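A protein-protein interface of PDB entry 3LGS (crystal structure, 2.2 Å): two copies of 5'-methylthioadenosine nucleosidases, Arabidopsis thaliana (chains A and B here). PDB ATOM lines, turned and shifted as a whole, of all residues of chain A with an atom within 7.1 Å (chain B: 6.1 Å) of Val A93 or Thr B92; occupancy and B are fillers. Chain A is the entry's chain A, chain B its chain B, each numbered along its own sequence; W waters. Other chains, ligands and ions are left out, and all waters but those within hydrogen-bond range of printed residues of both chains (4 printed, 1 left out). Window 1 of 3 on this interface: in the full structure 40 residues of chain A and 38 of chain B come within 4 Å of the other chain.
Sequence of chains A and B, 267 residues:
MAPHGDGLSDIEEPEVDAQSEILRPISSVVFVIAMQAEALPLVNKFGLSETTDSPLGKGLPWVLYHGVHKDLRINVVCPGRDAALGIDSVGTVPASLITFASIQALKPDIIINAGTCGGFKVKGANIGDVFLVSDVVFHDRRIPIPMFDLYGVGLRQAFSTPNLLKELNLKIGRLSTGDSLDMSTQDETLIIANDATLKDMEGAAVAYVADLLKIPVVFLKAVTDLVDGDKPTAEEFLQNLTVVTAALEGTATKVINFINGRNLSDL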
ATOM      1  N   TRP A  62      15.580 -32.520 -25.375  1.00  0.00           N
ATOM      2  CA  TRP A  62      15.740 -31.294 -26.149  1.00  0.00           C
ATOM      3  C   TRP A  62      15.792 -31.558 -27.641  1.00  0.00           C
ATOM      4  O   TRP A  62      16.432 -32.508 -28.104  1.00  0.00           O
ATOM      5  CB  TRP A  62      16.992 -30.520 -25.734  1.00  0.00           C
ATOM      6  CG  TRP A  62      17.100 -30.221 -24.257  1.00  0.00           C
ATOM      7  CD1 TRP A  62      16.099 -30.275 -23.323  1.00  0.00           C
ATOM      8  CD2 TRP A  62      18.285 -29.806 -23.551  1.00  0.00           C
ATOM      9  NE1 TRP A  62      16.587 -29.925 -22.088  1.00  0.00           N
ATOM     10  CE2 TRP A  62      17.925 -29.637 -22.197  1.00  0.00           C
ATOM     11  CE3 TRP A  62      19.614 -29.566 -23.934  1.00  0.00           C
ATOM     12  CZ2 TRP A  62      18.846 -29.234 -21.218  1.00  0.00           C
ATOM     13  CZ3 TRP A  62      20.535 -29.170 -22.952  1.00  0.00           C
ATOM     14  CH2 TRP A  62      20.144 -29.009 -21.613  1.00  0.00           C
ATOM     15  N   PRO A  79      12.978 -27.020 -25.460  1.00  0.00           N
ATOM     16  CA  PRO A  79      13.239 -27.801 -24.240  1.00  0.00           C
ATOM     17  C   PRO A  79      12.676 -29.208 -24.298  1.00  0.00           C
ATOM     18  O   PRO A  79      12.912 -30.009 -23.400  1.00  0.00           O
ATOM     19  CB  PRO A  79      12.510 -27.013 -23.144  1.00  0.00           C
ATOM     20  CG  PRO A  79      11.406 -26.323 -23.875  1.00  0.00           C
ATOM     21  CD  PRO A  79      11.992 -25.954 -25.217  1.00  0.00           C
ATOM     22  N   SER A  89       8.172 -28.772 -22.181  1.00  0.00           N
ATOM     23  CA  SER A  89       8.808 -28.502 -20.897  1.00  0.00           C
ATOM     24  C   SER A  89       8.970 -26.994 -20.768  1.00  0.00           C
ATOM     25  O   SER A  89      10.041 -26.457 -20.988  1.00  0.00           O
ATOM     26  CB  SER A  89      10.159 -29.221 -20.773  1.00  0.00           C
ATOM     27  OG  SER A  89      10.054 -30.597 -21.114  1.00  0.00           O
ATOM     28  N   VAL A  90       7.881 -26.327 -20.429  1.00  0.00           N
ATOM     29  CA  VAL A  90       7.841 -24.867 -20.285  1.00  0.00           C
ATOM     30  C   VAL A  90       8.489 -24.410 -18.970  1.00  0.00           C
ATOM     31  O   VAL A  90       8.826 -25.232 -18.101  1.00  0.00           O
ATOM     32  CB  VAL A  90       6.367 -24.334 -20.391  1.00  0.00           C
ATOM     33  CG1 VAL A  90       5.750 -24.627 -21.816  1.00  0.00           C
ATOM     34  CG2 VAL A  90       5.511 -24.925 -19.287  1.00  0.00           C
ATOM     35  N   GLY A  91       8.673 -23.100 -18.841  1.00  0.00           N
ATOM     36  CA  GLY A  91       9.210 -22.502 -17.635  1.00  0.00           C
ATOM     37  C   GLY A  91      10.658 -22.068 -17.763  1.00  0.00           C
ATOM     38  O   GLY A  91      11.341 -22.392 -18.740  1.00  0.00           O
ATOM     39  N   THR A  92      11.121 -21.325 -16.758  1.00  0.00           N
ATOM     40  CA  THR A  92      12.445 -20.713 -16.764  1.00  0.00           C
ATOM     41  C   THR A  92      13.594 -21.689 -16.707  1.00  0.00           C
ATOM     42  O   THR A  92      14.631 -21.423 -17.307  1.00  0.00           O
ATOM     43  CB  THR A  92      12.626 -19.736 -15.582  1.00  0.00           C
ATOM     44  OG1 THR A  92      12.474 -20.454 -14.344  1.00  0.00           O
ATOM     45  CG2 THR A  92      11.615 -18.571 -15.675  1.00  0.00           C
ATOM     46  N   VAL A  93      13.443 -22.804 -15.982  1.00  0.00           N
ATOM     47  CA  VAL A  93      14.588 -23.717 -15.816  1.00  0.00           C
ATOM     48  C   VAL A  93      14.996 -24.394 -17.151  1.00  0.00           C
ATOM     49  O   VAL A  93      16.150 -24.285 -17.567  1.00  0.00           O
ATOM     50  CB  VAL A  93      14.393 -24.740 -14.638  1.00  0.00           C
ATOM     51  CG1 VAL A  93      15.315 -25.963 -14.791  1.00  0.00           C
ATOM     52  CG2 VAL A  93      14.638 -24.077 -13.308  1.00  0.00           C
ATOM     53  N   PRO A  94      14.045 -25.067 -17.834  1.00  0.00           N
ATOM     54  CA  PRO A  94      14.381 -25.718 -19.112  1.00  0.00           C
ATOM     55  C   PRO A  94      14.827 -24.723 -20.204  1.00  0.00           C
ATOM     56  O   PRO A  94      15.765 -24.993 -20.955  1.00  0.00           O
ATOM     57  CB  PRO A  94      13.079 -26.430 -19.493  1.00  0.00           C
ATOM     58  CG  PRO A  94      12.326 -26.577 -18.176  1.00  0.00           C
ATOM     59  CD  PRO A  94      12.656 -25.348 -17.418  1.00  0.00           C
ATOM     60  N   ALA A  95      14.196 -23.562 -20.262  1.00  0.00           N
ATOM     61  CA  ALA A  95      14.599 -22.529 -21.210  1.00  0.00           C
ATOM     62  C   ALA A  95      16.044 -22.069 -20.953  1.00  0.00           C
ATOM     63  O   ALA A  95      16.834 -21.839 -21.878  1.00  0.00           O
ATOM     64  CB  ALA A  95      13.647 -21.362 -21.123  1.00  0.00           C
ATOM     65  N   SER A  96      16.383 -21.958 -19.675  1.00  0.00           N
ATOM     66  CA  SER A  96      17.673 -21.410 -19.306  1.00  0.00           C
ATOM     67  C   SER A  96      18.768 -22.457 -19.555  1.00  0.00           C
ATOM     68  O   SER A  96      19.884 -22.107 -19.928  1.00  0.00           O
ATOM     69  CB  SER A  96      17.647 -20.893 -17.866  1.00  0.00           C
ATOM     70  OG  SER A  96      18.111 -21.890 -16.977  1.00  0.00           O
ATOM     71  N   LEU A  97      18.431 -23.732 -19.371  1.00  0.00           N
ATOM     72  CA  LEU A  97      19.326 -24.830 -19.745  1.00  0.00           C
ATOM     73  C   LEU A  97      19.642 -24.870 -21.246  1.00  0.00           C
ATOM     74  O   LEU A  97      20.815 -24.947 -21.623  1.00  0.00           O
ATOM     75  CB  LEU A  97      18.762 -26.177 -19.291  1.00  0.00           C
ATOM     76  CG  LEU A  97      18.636 -26.343 -17.768  1.00  0.00           C
ATOM     77  CD1 LEU A  97      17.784 -27.547 -17.385  1.00  0.00           C
ATOM     78  CD2 LEU A  97      20.012 -26.440 -17.113  1.00  0.00           C
ATOM     79  N   ILE A  98      18.607 -24.830 -22.094  1.00  0.00           N
ATOM     80  CA  ILE A  98      18.830 -24.880 -23.548  1.00  0.00           C
ATOM     81  C   ILE A  98      19.537 -23.643 -24.072  1.00  0.00           C
ATOM     82  O   ILE A  98      20.358 -23.745 -24.978  1.00  0.00           O
ATOM     83  CB  ILE A  98      17.543 -25.182 -24.393  1.00  0.00           C
ATOM     84  CG1 ILE A  98      16.448 -24.134 -24.182  1.00  0.00           C
ATOM     85  CG2 ILE A  98      17.024 -26.558 -24.077  1.00  0.00           C
ATOM     86  CD1 ILE A  98      15.201 -24.362 -25.053  1.00  0.00           C
ATOM     87  N   THR A  99      19.227 -22.478 -23.508  1.00  0.00           N
ATOM     88  CA  THR A  99      19.950 -21.258 -23.840  1.00  0.00           C
ATOM     89  C   THR A  99      21.437 -21.497 -23.555  1.00  0.00           C
ATOM     90  O   THR A  99      22.293 -21.358 -24.451  1.00  0.00           O
ATOM     91  CB  THR A  99      19.390 -20.056 -23.054  1.00  0.00           C
ATOM     92  OG1 THR A  99      17.999 -19.934 -23.352  1.00  0.00           O
ATOM     93  CG2 THR A  99      20.068 -18.752 -23.451  1.00  0.00           C
ATOM     94  N   ARG A 141      10.420 -13.777  -8.186  1.00  0.00           N
ATOM     95  CA  ARG A 141      11.603 -14.020  -7.385  1.00  0.00           C
ATOM     96  C   ARG A 141      11.697 -12.913  -6.358  1.00  0.00           C
ATOM     97  O   ARG A 141      12.518 -11.992  -6.489  1.00  0.00           O
ATOM     98  CB  ARG A 141      12.863 -13.981  -8.218  1.00  0.00           C
ATOM     99  CG  ARG A 141      12.959 -14.880  -9.431  1.00  0.00           C
ATOM    100  CD  ARG A 141      14.103 -14.280 -10.197  1.00  0.00           C
ATOM    101  NE  ARG A 141      15.092 -15.246 -10.579  1.00  0.00           N
ATOM    102  CZ  ARG A 141      16.315 -14.939 -10.988  1.00  0.00           C
ATOM    103  NH1 ARG A 141      16.717 -13.679 -11.058  1.00  0.00           N
ATOM    104  NH2 ARG A 141      17.133 -15.919 -11.326  1.00  0.00           N
ATOM    105  N   TYR A 151      18.527  -8.184  -7.633  1.00  0.00           N
ATOM    106  CA  TYR A 151      18.940  -9.420  -8.238  1.00  0.00           C
ATOM    107  C   TYR A 151      17.730 -10.310  -8.645  1.00  0.00           C
ATOM    108  O   TYR A 151      17.634 -10.742  -9.782  1.00  0.00           O
ATOM    109  CB  TYR A 151      19.855 -10.177  -7.283  1.00  0.00           C
ATOM    110  CG  TYR A 151      20.052 -11.603  -7.723  1.00  0.00           C
ATOM    111  CD1 TYR A 151      20.925 -11.909  -8.765  1.00  0.00           C
ATOM    112  CD2 TYR A 151      19.348 -12.640  -7.119  1.00  0.00           C
ATOM    113  CE1 TYR A 151      21.105 -13.219  -9.190  1.00  0.00           C
ATOM    114  CE2 TYR A 151      19.515 -13.956  -7.538  1.00  0.00           C
ATOM    115  CZ  TYR A 151      20.388 -14.241  -8.569  1.00  0.00           C
ATOM    116  OH  TYR A 151      20.561 -15.536  -8.976  1.00  0.00           O
ATOM    117  N   ASP A 179       7.151 -18.406 -13.449  1.00  0.00           N
ATOM    118  CA  ASP A 179       6.935 -19.803 -13.835  1.00  0.00           C
ATOM    119  C   ASP A 179       5.471 -20.243 -13.765  1.00  0.00           C
ATOM    120  O   ASP A 179       5.184 -21.424 -13.939  1.00  0.00           O
ATOM    121  CB  ASP A 179       7.814 -20.742 -13.005  1.00  0.00           C
ATOM    122  CG  ASP A 179       9.223 -20.803 -13.513  1.00  0.00           C
ATOM    123  OD1 ASP A 179       9.453 -21.541 -14.506  1.00  0.00           O
ATOM    124  OD2 ASP A 179      10.100 -20.126 -12.911  1.00  0.00           O
ATOM    125  N   MET A 201       6.678 -16.916 -19.457  1.00  0.00           N
ATOM    126  CA  MET A 201       7.241 -17.908 -18.536  1.00  0.00           C
ATOM    127  C   MET A 201       8.748 -18.252 -18.660  1.00  0.00           C
ATOM    128  O   MET A 201       9.212 -19.155 -17.961  1.00  0.00           O
ATOM    129  CB  MET A 201       6.391 -19.181 -18.571  1.00  0.00           C
ATOM    130  CG  MET A 201       4.957 -18.990 -18.061  1.00  0.00           C
ATOM    131  SD  MET A 201       3.860 -20.387 -18.409  1.00  0.00           S
ATOM    132  CE  MET A 201       4.646 -21.644 -17.400  1.00  0.00           C
ATOM    133  N   GLU A 202       9.509 -17.539 -19.503  1.00  0.00           N
ATOM    134  CA  GLU A 202      10.932 -17.852 -19.697  1.00  0.00           C
ATOM    135  C   GLU A 202      11.823 -16.630 -19.918  1.00  0.00           C
ATOM    136  O   GLU A 202      13.012 -16.648 -19.585  1.00  0.00           O
ATOM    137  CB  GLU A 202      11.122 -18.853 -20.858  1.00  0.00           C
ATOM    138  CG  GLU A 202      11.002 -18.277 -22.282  1.00  0.00           C
ATOM    139  CD  GLU A 202       9.691 -18.629 -22.967  1.00  0.00           C
ATOM    140  OE1 GLU A 202       8.819 -19.235 -22.315  1.00  0.00           O
ATOM    141  OE2 GLU A 202       9.531 -18.309 -24.164  1.00  0.00           O
ATOM    142  N   ALA A 205      14.771 -15.300 -17.841  1.00  0.00           N
ATOM    143  CA  ALA A 205      15.778 -16.340 -17.588  1.00  0.00           C
ATOM    144  C   ALA A 205      16.665 -16.542 -18.794  1.00  0.00           C
ATOM    145  O   ALA A 205      17.855 -16.789 -18.637  1.00  0.00           O
ATOM    146  CB  ALA A 205      15.119 -17.657 -17.186  1.00  0.00           C
ATOM    147  N   VAL B  90      21.461 -16.845  -6.139  1.00  0.00           N
ATOM    148  CA  VAL B  90      20.538 -17.853  -5.639  1.00  0.00           C
ATOM    149  C   VAL B  90      19.353 -18.099  -6.610  1.00  0.00           C
ATOM    150  O   VAL B  90      19.226 -17.432  -7.652  1.00  0.00           O
ATOM    151  CB  VAL B  90      20.026 -17.449  -4.228  1.00  0.00           C
ATOM    152  CG1 VAL B  90      21.177 -17.459  -3.206  1.00  0.00           C
ATOM    153  CG2 VAL B  90      19.387 -16.088  -4.268  1.00  0.00           C
ATOM    154  N   GLY B  91      18.499 -19.057  -6.276  1.00  0.00           N
ATOM    155  CA  GLY B  91      17.314 -19.317  -7.080  1.00  0.00           C
ATOM    156  C   GLY B  91      17.446 -20.532  -7.996  1.00  0.00           C
ATOM    157  O   GLY B  91      18.510 -21.116  -8.129  1.00  0.00           O
ATOM    158  N   THR B  92      16.345 -20.920  -8.623  1.00  0.00           N
ATOM    159  CA  THR B  92      16.311 -22.157  -9.407  1.00  0.00           C
ATOM    160  C   THR B  92      17.168 -22.115 -10.656  1.00  0.00           C
ATOM    161  O   THR B  92      17.852 -23.071 -10.959  1.00  0.00           O
ATOM    162  CB  THR B  92      14.897 -22.508  -9.771  1.00  0.00           C
ATOM    163  OG1 THR B  92      14.328 -21.419 -10.517  1.00  0.00           O
ATOM    164  CG2 THR B  92      14.098 -22.774  -8.469  1.00  0.00           C
ATOM    165  N   VAL B  93      17.159 -21.003 -11.373  1.00  0.00           N
ATOM    166  CA  VAL B  93      17.905 -20.948 -12.640  1.00  0.00           C
ATOM    167  C   VAL B  93      19.432 -21.171 -12.481  1.00  0.00           C
ATOM    168  O   VAL B  93      19.984 -22.075 -13.112  1.00  0.00           O
ATOM    169  CB  VAL B  93      17.522 -19.698 -13.492  1.00  0.00           C
ATOM    170  CG1 VAL B  93      18.570 -19.418 -14.568  1.00  0.00           C
ATOM    171  CG2 VAL B  93      16.121 -19.878 -14.100  1.00  0.00           C
ATOM    172  N   PRO B  94      20.111 -20.374 -11.627  1.00  0.00           N
ATOM    173  CA  PRO B  94      21.549 -20.634 -11.441  1.00  0.00           C
ATOM    174  C   PRO B  94      21.826 -22.025 -10.855  1.00  0.00           C
ATOM    175  O   PRO B  94      22.752 -22.705 -11.309  1.00  0.00           O
ATOM    176  CB  PRO B  94      21.992 -19.532 -10.476  1.00  0.00           C
ATOM    177  CG  PRO B  94      20.926 -18.472 -10.600  1.00  0.00           C
ATOM    178  CD  PRO B  94      19.660 -19.207 -10.854  1.00  0.00           C
ATOM    179  N   ALA B  95      21.019 -22.471  -9.900  1.00  0.00           N
ATOM    180  CA  ALA B  95      21.220 -23.814  -9.365  1.00  0.00           C
ATOM    181  C   ALA B  95      21.050 -24.859 -10.471  1.00  0.00           C
ATOM    182  O   ALA B  95      21.774 -25.847 -10.510  1.00  0.00           O
ATOM    183  CB  ALA B  95      20.293 -24.091  -8.230  1.00  0.00           C
ATOM    184  N   SER B  96      20.116 -24.626 -11.389  1.00  0.00           N
ATOM    185  CA  SER B  96      19.869 -25.601 -12.421  1.00  0.00           C
ATOM    186  C   SER B  96      21.023 -25.618 -13.409  1.00  0.00           C
ATOM    187  O   SER B  96      21.445 -26.683 -13.842  1.00  0.00           O
ATOM    188  CB  SER B  96      18.512 -25.377 -13.097  1.00  0.00           C
ATOM    189  OG  SER B  96      18.605 -24.391 -14.120  1.00  0.00           O
ATOM    190  N   LEU B  97      21.555 -24.439 -13.730  1.00  0.00           N
ATOM    191  CA  LEU B  97      22.692 -24.312 -14.661  1.00  0.00           C
ATOM    192  C   LEU B  97      23.945 -25.049 -14.177  1.00  0.00           C
ATOM    193  O   LEU B  97      24.550 -25.813 -14.934  1.00  0.00           O
ATOM    194  CB  LEU B  97      22.995 -22.836 -14.961  1.00  0.00           C
ATOM    195  CG  LEU B  97      21.909 -22.037 -15.727  1.00  0.00           C
ATOM    196  CD1 LEU B  97      22.288 -20.595 -15.870  1.00  0.00           C
ATOM    197  CD2 LEU B  97      21.658 -22.629 -17.096  1.00  0.00           C
ATOM    198  N   PHE B 138       7.804 -28.116  -6.483  1.00  0.00           N
ATOM    199  CA  PHE B 138       7.761 -26.660  -6.645  1.00  0.00           C
ATOM    200  C   PHE B 138       6.408 -26.168  -6.103  1.00  0.00           C
ATOM    201  O   PHE B 138       5.374 -26.799  -6.365  1.00  0.00           O
ATOM    202  CB  PHE B 138       7.820 -26.277  -8.127  1.00  0.00           C
ATOM    203  CG  PHE B 138       9.146 -26.524  -8.813  1.00  0.00           C
ATOM    204  CD1 PHE B 138       9.381 -27.711  -9.508  1.00  0.00           C
ATOM    205  CD2 PHE B 138      10.112 -25.527  -8.866  1.00  0.00           C
ATOM    206  CE1 PHE B 138      10.579 -27.918 -10.202  1.00  0.00           C
ATOM    207  CE2 PHE B 138      11.328 -25.737  -9.539  1.00  0.00           C
ATOM    208  CZ  PHE B 138      11.554 -26.941 -10.214  1.00  0.00           C
ATOM    209  N   ASP B 140       5.715 -22.839  -6.814  1.00  0.00           N
ATOM    210  CA  ASP B 140       5.553 -21.588  -7.591  1.00  0.00           C
ATOM    211  C   ASP B 140       5.587 -21.740  -9.108  1.00  0.00           C
ATOM    212  O   ASP B 140       5.936 -20.792  -9.836  1.00  0.00           O
ATOM    213  CB  ASP B 140       6.566 -20.523  -7.123  1.00  0.00           C
ATOM    214  CG  ASP B 140       7.968 -20.689  -7.742  1.00  0.00           C
ATOM    215  OD1 ASP B 140       8.332 -21.806  -8.222  1.00  0.00           O
ATOM    216  OD2 ASP B 140       8.712 -19.678  -7.721  1.00  0.00           O
ATOM    217  N   ARG B 141       5.255 -22.939  -9.589  1.00  0.00           N
ATOM    218  CA  ARG B 141       5.085 -23.152 -11.022  1.00  0.00           C
ATOM    219  C   ARG B 141       3.634 -23.605 -11.252  1.00  0.00           C
ATOM    220  O   ARG B 141       3.369 -24.801 -11.434  1.00  0.00           O
ATOM    221  CB  ARG B 141       6.096 -24.170 -11.562  1.00  0.00           C
ATOM    222  CG  ARG B 141       7.533 -23.945 -11.093  1.00  0.00           C
ATOM    223  CD  ARG B 141       8.545 -24.541 -12.034  1.00  0.00           C
ATOM    224  NE  ARG B 141       8.300 -25.968 -12.259  1.00  0.00           N
ATOM    225  CZ  ARG B 141       9.034 -26.737 -13.067  1.00  0.00           C
ATOM    226  NH1 ARG B 141      10.072 -26.220 -13.714  1.00  0.00           N
ATOM    227  NH2 ARG B 141       8.732 -28.032 -13.219  1.00  0.00           N
ATOM    228  N   THR B 177      10.002 -26.067  -3.220  1.00  0.00           N
ATOM    229  CA  THR B 177      10.928 -25.101  -3.845  1.00  0.00           C
ATOM    230  C   THR B 177      10.175 -23.985  -4.558  1.00  0.00           C
ATOM    231  O   THR B 177       9.091 -24.210  -5.115  1.00  0.00           O
ATOM    232  CB  THR B 177      11.843 -25.849  -4.848  1.00  0.00           C
ATOM    233  OG1 THR B 177      12.704 -26.745  -4.125  1.00  0.00           O
ATOM    234  CG2 THR B 177      12.705 -24.881  -5.758  1.00  0.00           C
ATOM    235  N   GLY B 178      10.738 -22.783  -4.511  1.00  0.00           N
ATOM    236  CA  GLY B 178      10.231 -21.616  -5.231  1.00  0.00           C
ATOM    237  C   GLY B 178      11.285 -20.514  -5.194  1.00  0.00           C
ATOM    238  O   GLY B 178      12.145 -20.519  -4.315  1.00  0.00           O
ATOM    239  N   ASP B 179      11.222 -19.559  -6.128  1.00  0.00           N
ATOM    240  CA  ASP B 179      12.250 -18.510  -6.242  1.00  0.00           C
ATOM    241  C   ASP B 179      12.114 -17.297  -5.282  1.00  0.00           C
ATOM    242  O   ASP B 179      12.885 -16.339  -5.375  1.00  0.00           O
ATOM    243  CB  ASP B 179      12.387 -18.069  -7.711  1.00  0.00           C
ATOM    244  CG  ASP B 179      13.159 -19.089  -8.545  1.00  0.00           C
ATOM    245  OD1 ASP B 179      14.416 -19.061  -8.520  1.00  0.00           O
ATOM    246  OD2 ASP B 179      12.511 -19.948  -9.190  1.00  0.00           O
ATOM    247  N   MET B 201      14.844 -22.572  -2.161  1.00  0.00           N
ATOM    248  CA  MET B 201      14.865 -21.798  -3.411  1.00  0.00           C
ATOM    249  C   MET B 201      15.570 -22.487  -4.595  1.00  0.00           C
ATOM    250  O   MET B 201      15.739 -21.874  -5.659  1.00  0.00           O
ATOM    251  CB  MET B 201      15.480 -20.413  -3.181  1.00  0.00           C
ATOM    252  CG  MET B 201      14.590 -19.454  -2.421  1.00  0.00           C
ATOM    253  SD  MET B 201      15.476 -18.017  -1.760  1.00  0.00           S
ATOM    254  CE  MET B 201      15.784 -17.103  -3.267  1.00  0.00           C
ATOM    255  N   GLU B 202      15.965 -23.754  -4.447  1.00  0.00           N
ATOM    256  CA  GLU B 202      16.582 -24.437  -5.593  1.00  0.00           C
ATOM    257  C   GLU B 202      16.334 -25.936  -5.740  1.00  0.00           C
ATOM    258  O   GLU B 202      16.434 -26.453  -6.856  1.00  0.00           O
ATOM    259  CB  GLU B 202      18.094 -24.176  -5.643  1.00  0.00           C
ATOM    260  CG  GLU B 202      18.908 -25.039  -4.704  1.00  0.00           C
ATOM    261  CD  GLU B 202      19.466 -24.271  -3.514  1.00  0.00           C
ATOM    262  OE1 GLU B 202      19.103 -23.088  -3.327  1.00  0.00           O
ATOM    263  OE2 GLU B 202      20.288 -24.850  -2.770  1.00  0.00           O
ATOM    264  N   GLY B 203      16.052 -26.625  -4.627  1.00  0.00           N
ATOM    265  CA  GLY B 203      16.016 -28.092  -4.590  1.00  0.00           C
ATOM    266  C   GLY B 203      15.343 -28.792  -5.762  1.00  0.00           C
ATOM    267  O   GLY B 203      15.936 -29.667  -6.389  1.00  0.00           O
ATOM    268  N   ALA B 205      14.579 -27.769  -8.686  1.00  0.00           N
ATOM    269  CA  ALA B 205      15.275 -27.527  -9.957  1.00  0.00           C
ATOM    270  C   ALA B 205      16.516 -28.420 -10.082  1.00  0.00           C
ATOM    271  O   ALA B 205      16.796 -28.962 -11.163  1.00  0.00           O
ATOM    272  CB  ALA B 205      15.631 -26.060 -10.120  1.00  0.00           C
ATOM    273  N   VAL B 206      17.243 -28.600  -8.978  1.00  0.00           N
ATOM    274  CA  VAL B 206      18.348 -29.567  -8.941  1.00  0.00           C
ATOM    275  C   VAL B 206      17.836 -30.981  -9.285  1.00  0.00           C
ATOM    276  O   VAL B 206      18.457 -31.702 -10.080  1.00  0.00           O
ATOM    277  CB  VAL B 206      19.085 -29.562  -7.560  1.00  0.00           C
ATOM    278  CG1 VAL B 206      20.099 -30.699  -7.486  1.00  0.00           C
ATOM    279  CG2 VAL B 206      19.768 -28.195  -7.308  1.00  0.00           C
ATOM    280  N   TYR B 208      15.174 -31.822 -11.007  1.00  0.00           N
ATOM    281  CA  TYR B 208      14.755 -31.879 -12.404  1.00  0.00           C
ATOM    282  C   TYR B 208      15.955 -32.168 -13.311  1.00  0.00           C
ATOM    283  O   TYR B 208      15.889 -33.014 -14.208  1.00  0.00           O
ATOM    284  CB  TYR B 208      14.080 -30.574 -12.828  1.00  0.00           C
ATOM    285  CG  TYR B 208      13.746 -30.542 -14.299  1.00  0.00           C
ATOM    286  CD1 TYR B 208      12.660 -31.266 -14.804  1.00  0.00           C
ATOM    287  CD2 TYR B 208      14.527 -29.801 -15.195  1.00  0.00           C
ATOM    288  CE1 TYR B 208      12.357 -31.238 -16.167  1.00  0.00           C
ATOM    289  CE2 TYR B 208      14.234 -29.771 -16.553  1.00  0.00           C
ATOM    290  CZ  TYR B 208      13.151 -30.488 -17.032  1.00  0.00           C
ATOM    291  OH  TYR B 208      12.851 -30.449 -18.376  1.00  0.00           O
ATOM    292  N   VAL B 209      17.048 -31.457 -13.078  1.00  0.00           N
ATOM    293  CA  VAL B 209      18.246 -31.628 -13.890  1.00  0.00           C
ATOM    294  C   VAL B 209      18.862 -33.018 -13.661  1.00  0.00           C
ATOM    295  O   VAL B 209      19.192 -33.718 -14.613  1.00  0.00           O
ATOM    296  CB  VAL B 209      19.276 -30.509 -13.624  1.00  0.00           C
ATOM    297  CG1 VAL B 209      20.521 -30.752 -14.430  1.00  0.00           C
ATOM    298  CG2 VAL B 209      18.675 -29.150 -14.002  1.00  0.00           C
HETATM  299  O   HOH W   1      10.849 -32.116 -19.097  1.00  0.00           O
HETATM  300  O   HOH W   2      15.690 -18.316 -10.730  1.00  0.00           O
HETATM  301  O   HOH W   3      14.036 -29.819 -20.689  1.00  0.00           O
HETATM  302  O   HOH W   4      11.171 -23.517 -14.048  1.00  0.00           O
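Printed residues of chain B within 4 Å of Pro A94: Tyr B208.
Printed residues of chain B within 4 Å of Asp A179: Asp B140 and Arg B141.
Of the printed residues of chain A, Val B90 touches Tyr A151.
Thr B92 touches just one residue of chain A: Val A93.
Printed residues of chain A within 4 Å of Ser B96: Val A93 (3.7 Å), Ser A96 (3.8 Å) and Leu A97 (3.6 Å).
Printed residues of chain A within 4 Å of Asp B140: Asp A179 (3.7 Å).
Met B201 touches none of the printed residues of chain A.
The nearest printed residue of chain A that does not touch Leu B97 is Leu A97 (4.1 Å).
Of the 21 printed residues of chain B, 12 touch a printed residue of chain A.
Of the 19 printed residues of chain A, 10 touch a printed residue of chain B.
Among the printed residues, 18 pairs touch across the chains.
Among the printed residues, no Asp or Glu carboxylate lies within 4 Å of a Lys or Arg side-chain nitrogen of the other chain.
Val A93 touches Ser B96, and with the chains exchanged Ser A96 touches Val B93.
Val A93 touches Ala B205, and with the chains exchanged Ala A205 touches Val B93.
Ser B96 touches its own counterpart, Ser A96.
Arg A141 touches Asp B179, and with the chains exchanged Asp A179 touches Arg B141.
Positions printed for both chains: 90, 91, 92, 93, 94, 95, 96, 97, 141, 179, 201, 202 and 205.
Of the 18 pairs that touch across the chains among the printed residues, 11 have their exchanged pair printed and touching as well.
Tyr B208 touches Ser A89 (OH to CB, 3.8 Å).
OG1 of Thr A92 touches CG2 of Val B93 (3.7 Å).
CB of Ser B96 touches CG1 of Val A93, at 3.7 Å.
Ala B205 touches Val A93.
CG1 of Val A93 touches CD2 of Tyr B208 (3.9 Å).
Pro A94 touches Tyr B208.
O of Ser A96 touches CD2 of Leu B97 (3.4 Å).
Leu A97 touches Ser B96 (CD2 to O, 3.6 Å).
Leu A97 touches Val B209 (CD1 to CG2, 3.8 Å).
CB of Asp A179 touches O of Asp B140, 3.7 Å away.
Water W1 lies within hydrogen-bond range of the side-chain hydroxyl (OG) of Ser A89 and the side-chain hydroxyl (OH) of Tyr B208.
Water W4 lies within hydrogen-bond range of the side-chain carboxylate of Asp A179 (2.7 Å), the guanidinium group of Arg B141 (2.9 Å), the backbone NH of Val A93 (3.1 Å) and the side-chain hydroxyl of Thr A92 (3.3 Å).
Water W3 lies within hydrogen-bond range of OH of Tyr B208 (2.7 Å), NE1 of Trp A62 (2.9 Å) and O of Pro A79 (2.9 Å).
The backbone carbonyl oxygen (O) of Val B90 sits at hydrogen-bond distance from the side-chain hydroxyl (OH) of Tyr A151 (2.7 Å).
O of Tyr A151 lies within hydrogen-bond range of NH1 of Arg A141, 3.3 Å away.
The side-chain carboxylate (OD1) of Asp B179 is in hydrogen-bond range of the backbone NH (N) of Thr B92 (2.7 Å).
The backbone NH (N) of Thr A92 is in hydrogen-bond range of the backbone carbonyl oxygen (O) of Met A201 (3.1 Å).
The backbone carbonyl oxygen of Val A93 is in hydrogen-bond range of the side-chain hydroxyl of Ser A96 (3.2 Å).
O of Val B93 lies within hydrogen-bond range of OG of Ser B96.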
